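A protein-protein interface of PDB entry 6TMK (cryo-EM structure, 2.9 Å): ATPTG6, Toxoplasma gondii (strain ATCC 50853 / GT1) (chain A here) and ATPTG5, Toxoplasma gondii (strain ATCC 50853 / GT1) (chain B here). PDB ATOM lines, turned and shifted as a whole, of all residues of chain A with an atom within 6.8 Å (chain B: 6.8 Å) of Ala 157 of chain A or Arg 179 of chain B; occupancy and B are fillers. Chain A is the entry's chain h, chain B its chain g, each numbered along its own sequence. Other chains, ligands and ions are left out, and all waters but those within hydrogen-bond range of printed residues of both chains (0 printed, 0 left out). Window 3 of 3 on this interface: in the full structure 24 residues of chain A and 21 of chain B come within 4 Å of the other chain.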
ATOM      1  N   VAL A 152     -27.681  -9.822   8.628  1.00  0.00           N
ATOM      2  CA  VAL A 152     -29.120  -9.839   8.844  1.00  0.00           C
ATOM      3  C   VAL A 152     -29.473  -9.197  10.174  1.00  0.00           C
ATOM      4  O   VAL A 152     -30.448  -8.447  10.275  1.00  0.00           O
ATOM      5  CB  VAL A 152     -29.648 -11.281   8.764  1.00  0.00           C
ATOM      6  CG1 VAL A 152     -31.070 -11.349   9.246  1.00  0.00           C
ATOM      7  CG2 VAL A 152     -29.536 -11.812   7.360  1.00  0.00           C
ATOM      8  N   ASN A 153     -28.689  -9.472  11.213  1.00  0.00           N
ATOM      9  CA  ASN A 153     -29.019  -8.945  12.529  1.00  0.00           C
ATOM     10  C   ASN A 153     -28.776  -7.446  12.602  1.00  0.00           C
ATOM     11  O   ASN A 153     -29.552  -6.718  13.233  1.00  0.00           O
ATOM     12  CB  ASN A 153     -28.228  -9.694  13.595  1.00  0.00           C
ATOM     13  CG  ASN A 153     -28.583 -11.162  13.649  1.00  0.00           C
ATOM     14  OD1 ASN A 153     -29.721 -11.546  13.400  1.00  0.00           O
ATOM     15  ND2 ASN A 153     -27.613 -11.987  13.984  1.00  0.00           N
ATOM     16  N   ASP A 154     -27.724  -6.957  11.944  1.00  0.00           N
ATOM     17  CA  ASP A 154     -27.514  -5.516  11.874  1.00  0.00           C
ATOM     18  C   ASP A 154     -28.662  -4.832  11.139  1.00  0.00           C
ATOM     19  O   ASP A 154     -29.180  -3.798  11.584  1.00  0.00           O
ATOM     20  CB  ASP A 154     -26.179  -5.220  11.193  1.00  0.00           C
ATOM     21  CG  ASP A 154     -25.004  -5.314  12.148  1.00  0.00           C
ATOM     22  OD1 ASP A 154     -24.784  -4.356  12.919  1.00  0.00           O
ATOM     23  OD2 ASP A 154     -24.301  -6.347  12.133  1.00  0.00           O
ATOM     24  N   PHE A 155     -29.072  -5.401  10.004  1.00  0.00           N
ATOM     25  CA  PHE A 155     -30.183  -4.835   9.248  1.00  0.00           C
ATOM     26  C   PHE A 155     -31.468  -4.843  10.066  1.00  0.00           C
ATOM     27  O   PHE A 155     -32.241  -3.879  10.037  1.00  0.00           O
ATOM     28  CB  PHE A 155     -30.351  -5.613   7.943  1.00  0.00           C
ATOM     29  CG  PHE A 155     -31.496  -5.159   7.103  1.00  0.00           C
ATOM     30  CD1 PHE A 155     -31.394  -4.026   6.330  1.00  0.00           C
ATOM     31  CD2 PHE A 155     -32.672  -5.871   7.078  1.00  0.00           C
ATOM     32  CE1 PHE A 155     -32.441  -3.611   5.560  1.00  0.00           C
ATOM     33  CE2 PHE A 155     -33.720  -5.459   6.309  1.00  0.00           C
ATOM     34  CZ  PHE A 155     -33.608  -4.331   5.548  1.00  0.00           C
ATOM     35  N   ALA A 156     -31.711  -5.926  10.804  1.00  0.00           N
ATOM     36  CA  ALA A 156     -32.901  -6.010  11.638  1.00  0.00           C
ATOM     37  C   ALA A 156     -32.884  -4.953  12.730  1.00  0.00           C
ATOM     38  O   ALA A 156     -33.914  -4.337  13.027  1.00  0.00           O
ATOM     39  CB  ALA A 156     -33.005  -7.403  12.242  1.00  0.00           C
ATOM     40  N   ALA A 157     -31.726  -4.740  13.354  1.00  0.00           N
ATOM     41  CA  ALA A 157     -31.615  -3.694  14.360  1.00  0.00           C
ATOM     42  C   ALA A 157     -31.920  -2.329  13.762  1.00  0.00           C
ATOM     43  O   ALA A 157     -32.652  -1.528  14.357  1.00  0.00           O
ATOM     44  CB  ALA A 157     -30.220  -3.717  14.973  1.00  0.00           C
ATOM     45  N   LYS A 158     -31.363  -2.045  12.584  1.00  0.00           N
ATOM     46  CA  LYS A 158     -31.604  -0.753  11.952  1.00  0.00           C
ATOM     47  C   LYS A 158     -33.076  -0.569  11.611  1.00  0.00           C
ATOM     48  O   LYS A 158     -33.626   0.526  11.764  1.00  0.00           O
ATOM     49  CB  LYS A 158     -30.739  -0.611  10.703  1.00  0.00           C
ATOM     50  CG  LYS A 158     -29.261  -0.535  10.998  1.00  0.00           C
ATOM     51  CD  LYS A 158     -28.431  -0.502   9.739  1.00  0.00           C
ATOM     52  CE  LYS A 158     -26.953  -0.549  10.068  1.00  0.00           C
ATOM     53  NZ  LYS A 158     -26.230  -1.623   9.343  1.00  0.00           N
ATOM     54  N   VAL A 159     -33.741  -1.636  11.176  1.00  0.00           N
ATOM     55  CA  VAL A 159     -35.147  -1.519  10.803  1.00  0.00           C
ATOM     56  C   VAL A 159     -36.010  -1.313  12.041  1.00  0.00           C
ATOM     57  O   VAL A 159     -36.943  -0.496  12.044  1.00  0.00           O
ATOM     58  CB  VAL A 159     -35.577  -2.767  10.013  1.00  0.00           C
ATOM     59  CG1 VAL A 159     -37.071  -2.851   9.912  1.00  0.00           C
ATOM     60  CG2 VAL A 159     -34.970  -2.756   8.645  1.00  0.00           C
ATOM     61  N   HIS A 160     -35.710  -2.049  13.110  1.00  0.00           N
ATOM     62  CA  HIS A 160     -36.429  -1.871  14.362  1.00  0.00           C
ATOM     63  C   HIS A 160     -36.265  -0.457  14.894  1.00  0.00           C
ATOM     64  O   HIS A 160     -37.210   0.125  15.437  1.00  0.00           O
ATOM     65  CB  HIS A 160     -35.928  -2.883  15.384  1.00  0.00           C
ATOM     66  CG  HIS A 160     -36.795  -3.004  16.591  1.00  0.00           C
ATOM     67  ND1 HIS A 160     -38.145  -3.261  16.512  1.00  0.00           N
ATOM     68  CD2 HIS A 160     -36.509  -2.893  17.909  1.00  0.00           C
ATOM     69  CE1 HIS A 160     -38.652  -3.314  17.729  1.00  0.00           C
ATOM     70  NE2 HIS A 160     -37.680  -3.093  18.595  1.00  0.00           N
ATOM     71  N   ALA A 161     -35.067   0.111  14.754  1.00  0.00           N
ATOM     72  CA  ALA A 161     -34.864   1.501  15.144  1.00  0.00           C
ATOM     73  C   ALA A 161     -35.638   2.450  14.241  1.00  0.00           C
ATOM     74  O   ALA A 161     -36.160   3.468  14.706  1.00  0.00           O
ATOM     75  CB  ALA A 161     -33.378   1.835  15.113  1.00  0.00           C
ATOM     76  N   ASP A 162     -35.725   2.134  12.950  1.00  0.00           N
ATOM     77  CA  ASP A 162     -36.459   2.994  12.031  1.00  0.00           C
ATOM     78  C   ASP A 162     -37.922   3.085  12.431  1.00  0.00           C
ATOM     79  O   ASP A 162     -38.471   4.184  12.572  1.00  0.00           O
ATOM     80  CB  ASP A 162     -36.322   2.472  10.603  1.00  0.00           C
ATOM     81  CG  ASP A 162     -37.058   3.326   9.599  1.00  0.00           C
ATOM     82  OD1 ASP A 162     -36.769   4.537   9.521  1.00  0.00           O
ATOM     83  OD2 ASP A 162     -37.927   2.785   8.886  1.00  0.00           O
ATOM     84  N   ILE A 173     -37.219  -7.760   6.619  1.00  0.00           N
ATOM     85  CA  ILE A 173     -36.094  -8.533   7.139  1.00  0.00           C
ATOM     86  C   ILE A 173     -35.979  -9.871   6.420  1.00  0.00           C
ATOM     87  O   ILE A 173     -34.874 -10.364   6.171  1.00  0.00           O
ATOM     88  CB  ILE A 173     -36.228  -8.718   8.662  1.00  0.00           C
ATOM     89  CG1 ILE A 173     -35.993  -7.396   9.375  1.00  0.00           C
ATOM     90  CG2 ILE A 173     -35.231  -9.719   9.171  1.00  0.00           C
ATOM     91  CD1 ILE A 173     -36.677  -7.284  10.696  1.00  0.00           C
ATOM     92  N   GLN B 147     -23.518 -10.122  16.581  1.00  0.00           N
ATOM     93  CA  GLN B 147     -23.392  -8.875  15.850  1.00  0.00           C
ATOM     94  C   GLN B 147     -21.937  -8.443  15.824  1.00  0.00           C
ATOM     95  O   GLN B 147     -21.166  -8.728  16.743  1.00  0.00           O
ATOM     96  CB  GLN B 147     -24.262  -7.774  16.467  1.00  0.00           C
ATOM     97  CG  GLN B 147     -25.670  -7.725  15.907  1.00  0.00           C
ATOM     98  CD  GLN B 147     -26.488  -6.588  16.452  1.00  0.00           C
ATOM     99  OE1 GLN B 147     -26.146  -5.420  16.279  1.00  0.00           O
ATOM    100  NE2 GLN B 147     -27.589  -6.921  17.113  1.00  0.00           N
ATOM    101  N   PHE B 148     -21.573  -7.760  14.744  1.00  0.00           N
ATOM    102  CA  PHE B 148     -20.230  -7.214  14.583  1.00  0.00           C
ATOM    103  C   PHE B 148     -20.346  -6.116  13.537  1.00  0.00           C
ATOM    104  O   PHE B 148     -20.556  -6.407  12.356  1.00  0.00           O
ATOM    105  CB  PHE B 148     -19.251  -8.296  14.158  1.00  0.00           C
ATOM    106  CG  PHE B 148     -17.820  -7.881  14.236  1.00  0.00           C
ATOM    107  CD1 PHE B 148     -17.190  -7.760  15.454  1.00  0.00           C
ATOM    108  CD2 PHE B 148     -17.100  -7.620  13.090  1.00  0.00           C
ATOM    109  CE1 PHE B 148     -15.876  -7.381  15.529  1.00  0.00           C
ATOM    110  CE2 PHE B 148     -15.786  -7.242  13.161  1.00  0.00           C
ATOM    111  CZ  PHE B 148     -15.174  -7.124  14.383  1.00  0.00           C
ATOM    112  N   ASP B 149     -20.203  -4.868  13.968  1.00  0.00           N
ATOM    113  CA  ASP B 149     -20.496  -3.720  13.122  1.00  0.00           C
ATOM    114  C   ASP B 149     -19.257  -3.322  12.332  1.00  0.00           C
ATOM    115  O   ASP B 149     -18.217  -3.000  12.914  1.00  0.00           O
ATOM    116  CB  ASP B 149     -20.990  -2.545  13.965  1.00  0.00           C
ATOM    117  CG  ASP B 149     -22.033  -1.711  13.254  1.00  0.00           C
ATOM    118  OD1 ASP B 149     -22.176  -1.850  12.023  1.00  0.00           O
ATOM    119  OD2 ASP B 149     -22.709  -0.910  13.931  1.00  0.00           O
ATOM    120  N   ARG B 155     -18.631   5.455  11.405  1.00  0.00           N
ATOM    121  CA  ARG B 155     -19.681   6.272  12.000  1.00  0.00           C
ATOM    122  C   ARG B 155     -19.134   7.162  13.107  1.00  0.00           C
ATOM    123  O   ARG B 155     -19.476   8.347  13.196  1.00  0.00           O
ATOM    124  CB  ARG B 155     -20.772   5.361  12.539  1.00  0.00           C
ATOM    125  CG  ARG B 155     -21.868   6.051  13.296  1.00  0.00           C
ATOM    126  CD  ARG B 155     -23.052   5.142  13.393  1.00  0.00           C
ATOM    127  NE  ARG B 155     -22.647   3.791  13.763  1.00  0.00           N
ATOM    128  CZ  ARG B 155     -23.159   2.676  13.257  1.00  0.00           C
ATOM    129  NH1 ARG B 155     -24.114   2.719  12.345  1.00  0.00           N
ATOM    130  NH2 ARG B 155     -22.708   1.506  13.673  1.00  0.00           N
ATOM    131  N   PRO B 176     -13.525   0.856  21.003  1.00  0.00           N
ATOM    132  CA  PRO B 176     -14.060  -0.285  20.261  1.00  0.00           C
ATOM    133  C   PRO B 176     -15.506  -0.584  20.626  1.00  0.00           C
ATOM    134  O   PRO B 176     -16.003  -0.219  21.692  1.00  0.00           O
ATOM    135  CB  PRO B 176     -13.137  -1.429  20.682  1.00  0.00           C
ATOM    136  CG  PRO B 176     -12.744  -1.075  22.053  1.00  0.00           C
ATOM    137  CD  PRO B 176     -12.649   0.423  22.102  1.00  0.00           C
ATOM    138  N   ASP B 177     -16.178  -1.265  19.705  1.00  0.00           N
ATOM    139  CA  ASP B 177     -17.616  -1.456  19.819  1.00  0.00           C
ATOM    140  C   ASP B 177     -17.955  -2.355  20.996  1.00  0.00           C
ATOM    141  O   ASP B 177     -17.354  -3.417  21.178  1.00  0.00           O
ATOM    142  CB  ASP B 177     -18.171  -2.057  18.530  1.00  0.00           C
ATOM    143  CG  ASP B 177     -19.653  -1.810  18.364  1.00  0.00           C
ATOM    144  OD1 ASP B 177     -20.245  -1.126  19.223  1.00  0.00           O
ATOM    145  OD2 ASP B 177     -20.229  -2.305  17.373  1.00  0.00           O
ATOM    146  N   ALA B 178     -18.923  -1.921  21.796  1.00  0.00           N
ATOM    147  CA  ALA B 178     -19.530  -2.777  22.799  1.00  0.00           C
ATOM    148  C   ALA B 178     -20.683  -3.597  22.247  1.00  0.00           C
ATOM    149  O   ALA B 178     -21.045  -4.616  22.846  1.00  0.00           O
ATOM    150  CB  ALA B 178     -20.024  -1.933  23.973  1.00  0.00           C
ATOM    151  N   ARG B 179     -21.268  -3.178  21.125  1.00  0.00           N
ATOM    152  CA  ARG B 179     -22.345  -3.921  20.477  1.00  0.00           C
ATOM    153  C   ARG B 179     -21.760  -5.058  19.640  1.00  0.00           C
ATOM    154  O   ARG B 179     -21.789  -5.060  18.408  1.00  0.00           O
ATOM    155  CB  ARG B 179     -23.194  -2.990  19.629  1.00  0.00           C
ATOM    156  CG  ARG B 179     -24.161  -2.173  20.423  1.00  0.00           C
ATOM    157  CD  ARG B 179     -25.139  -1.451  19.537  1.00  0.00           C
ATOM    158  NE  ARG B 179     -26.142  -2.364  19.001  1.00  0.00           N
ATOM    159  CZ  ARG B 179     -26.136  -2.871  17.774  1.00  0.00           C
ATOM    160  NH1 ARG B 179     -25.177  -2.573  16.917  1.00  0.00           N
ATOM    161  NH2 ARG B 179     -27.101  -3.691  17.406  1.00  0.00           N
ATOM    162  N   VAL B 180     -21.221  -6.047  20.344  1.00  0.00           N
ATOM    163  CA  VAL B 180     -20.731  -7.265  19.716  1.00  0.00           C
ATOM    164  C   VAL B 180     -21.478  -8.433  20.334  1.00  0.00           C
ATOM    165  O   VAL B 180     -22.363  -8.243  21.174  1.00  0.00           O
ATOM    166  CB  VAL B 180     -19.210  -7.434  19.868  1.00  0.00           C
ATOM    167  CG1 VAL B 180     -18.483  -6.259  19.262  1.00  0.00           C
ATOM    168  CG2 VAL B 180     -18.835  -7.606  21.318  1.00  0.00           C
ATOM    169  N   THR B 181     -21.128  -9.641  19.926  1.00  0.00           N
ATOM    170  CA  THR B 181     -21.804 -10.810  20.451  1.00  0.00           C
ATOM    171  C   THR B 181     -21.604 -10.874  21.964  1.00  0.00           C
ATOM    172  O   THR B 181     -20.492 -10.640  22.450  1.00  0.00           O
ATOM    173  CB  THR B 181     -21.270 -12.077  19.792  1.00  0.00           C
ATOM    174  OG1 THR B 181     -21.265 -11.911  18.370  1.00  0.00           O
ATOM    175  CG2 THR B 181     -22.122 -13.261  20.157  1.00  0.00           C
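Of chain B, only Arg 179 comes within 4 Å of Ala 157 of chain A.
Of chain A, only Ala 157 (3.96 Å) comes within 4 Å of Arg 179 of chain B.
Printed residues of chain B within 4 Å of Asp 154 of chain A: Gln 147, Phe 148 and Asp 149.
Of the printed residues of chain A, Asp 149 of chain B touches Asp 154 (3.7 Å).
Printed residues of chain A within 4 Å of Phe 148 of chain B: Asp 154.
Val 180 of chain B touches none of the printed residues of chain A.
Ala 156 of chain A touches none of the printed residues of chain B.
The nearest residue of chain A that does not touch Arg 179 of chain B is Asp 154 of chain A (4.4 Å).
Of the 12 printed residues of chain A, 3 touch a printed residue of chain B.
Hydrophobic or aromatic side chains of chain A within 4 Å of the printed part of chain B: Ala 157.
Gln 147 of chain B touches Asn 153 of chain A (CG to CB, 3.97 Å).
Asp 154 of chain A touches Gln 147 of chain B (OD1 to OE1, 3.8 Å).
OD2 of Asp 154 of chain A touches O of Phe 148 of chain B, 3.8 Å away.
OD1 of Asp 149 of chain B touches OD1 of Asp 154 of chain A, 3.7 Å away.
CB of Ala 157 of chain A touches NH2 of Arg 179 of chain B, 3.96 Å away.
NH1 of Arg 179 of chain B sits close to OE1 of Gln 147 of chain B (3.1 Å).
O of Gln 147 of chain B is in hydrogen-bond range of N of Thr 181 of chain B.
The guanidinium group (NH2) of Arg 155 of chain B is in salt-bridge range of the side-chain carboxylate (OD2) of Asp 149 of chain B (2.4 Å).
The side-chain carboxylate (OD1) of Asp 177 of chain B sits at hydrogen-bond distance from the backbone NH (N) of Arg 179 of chain B.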
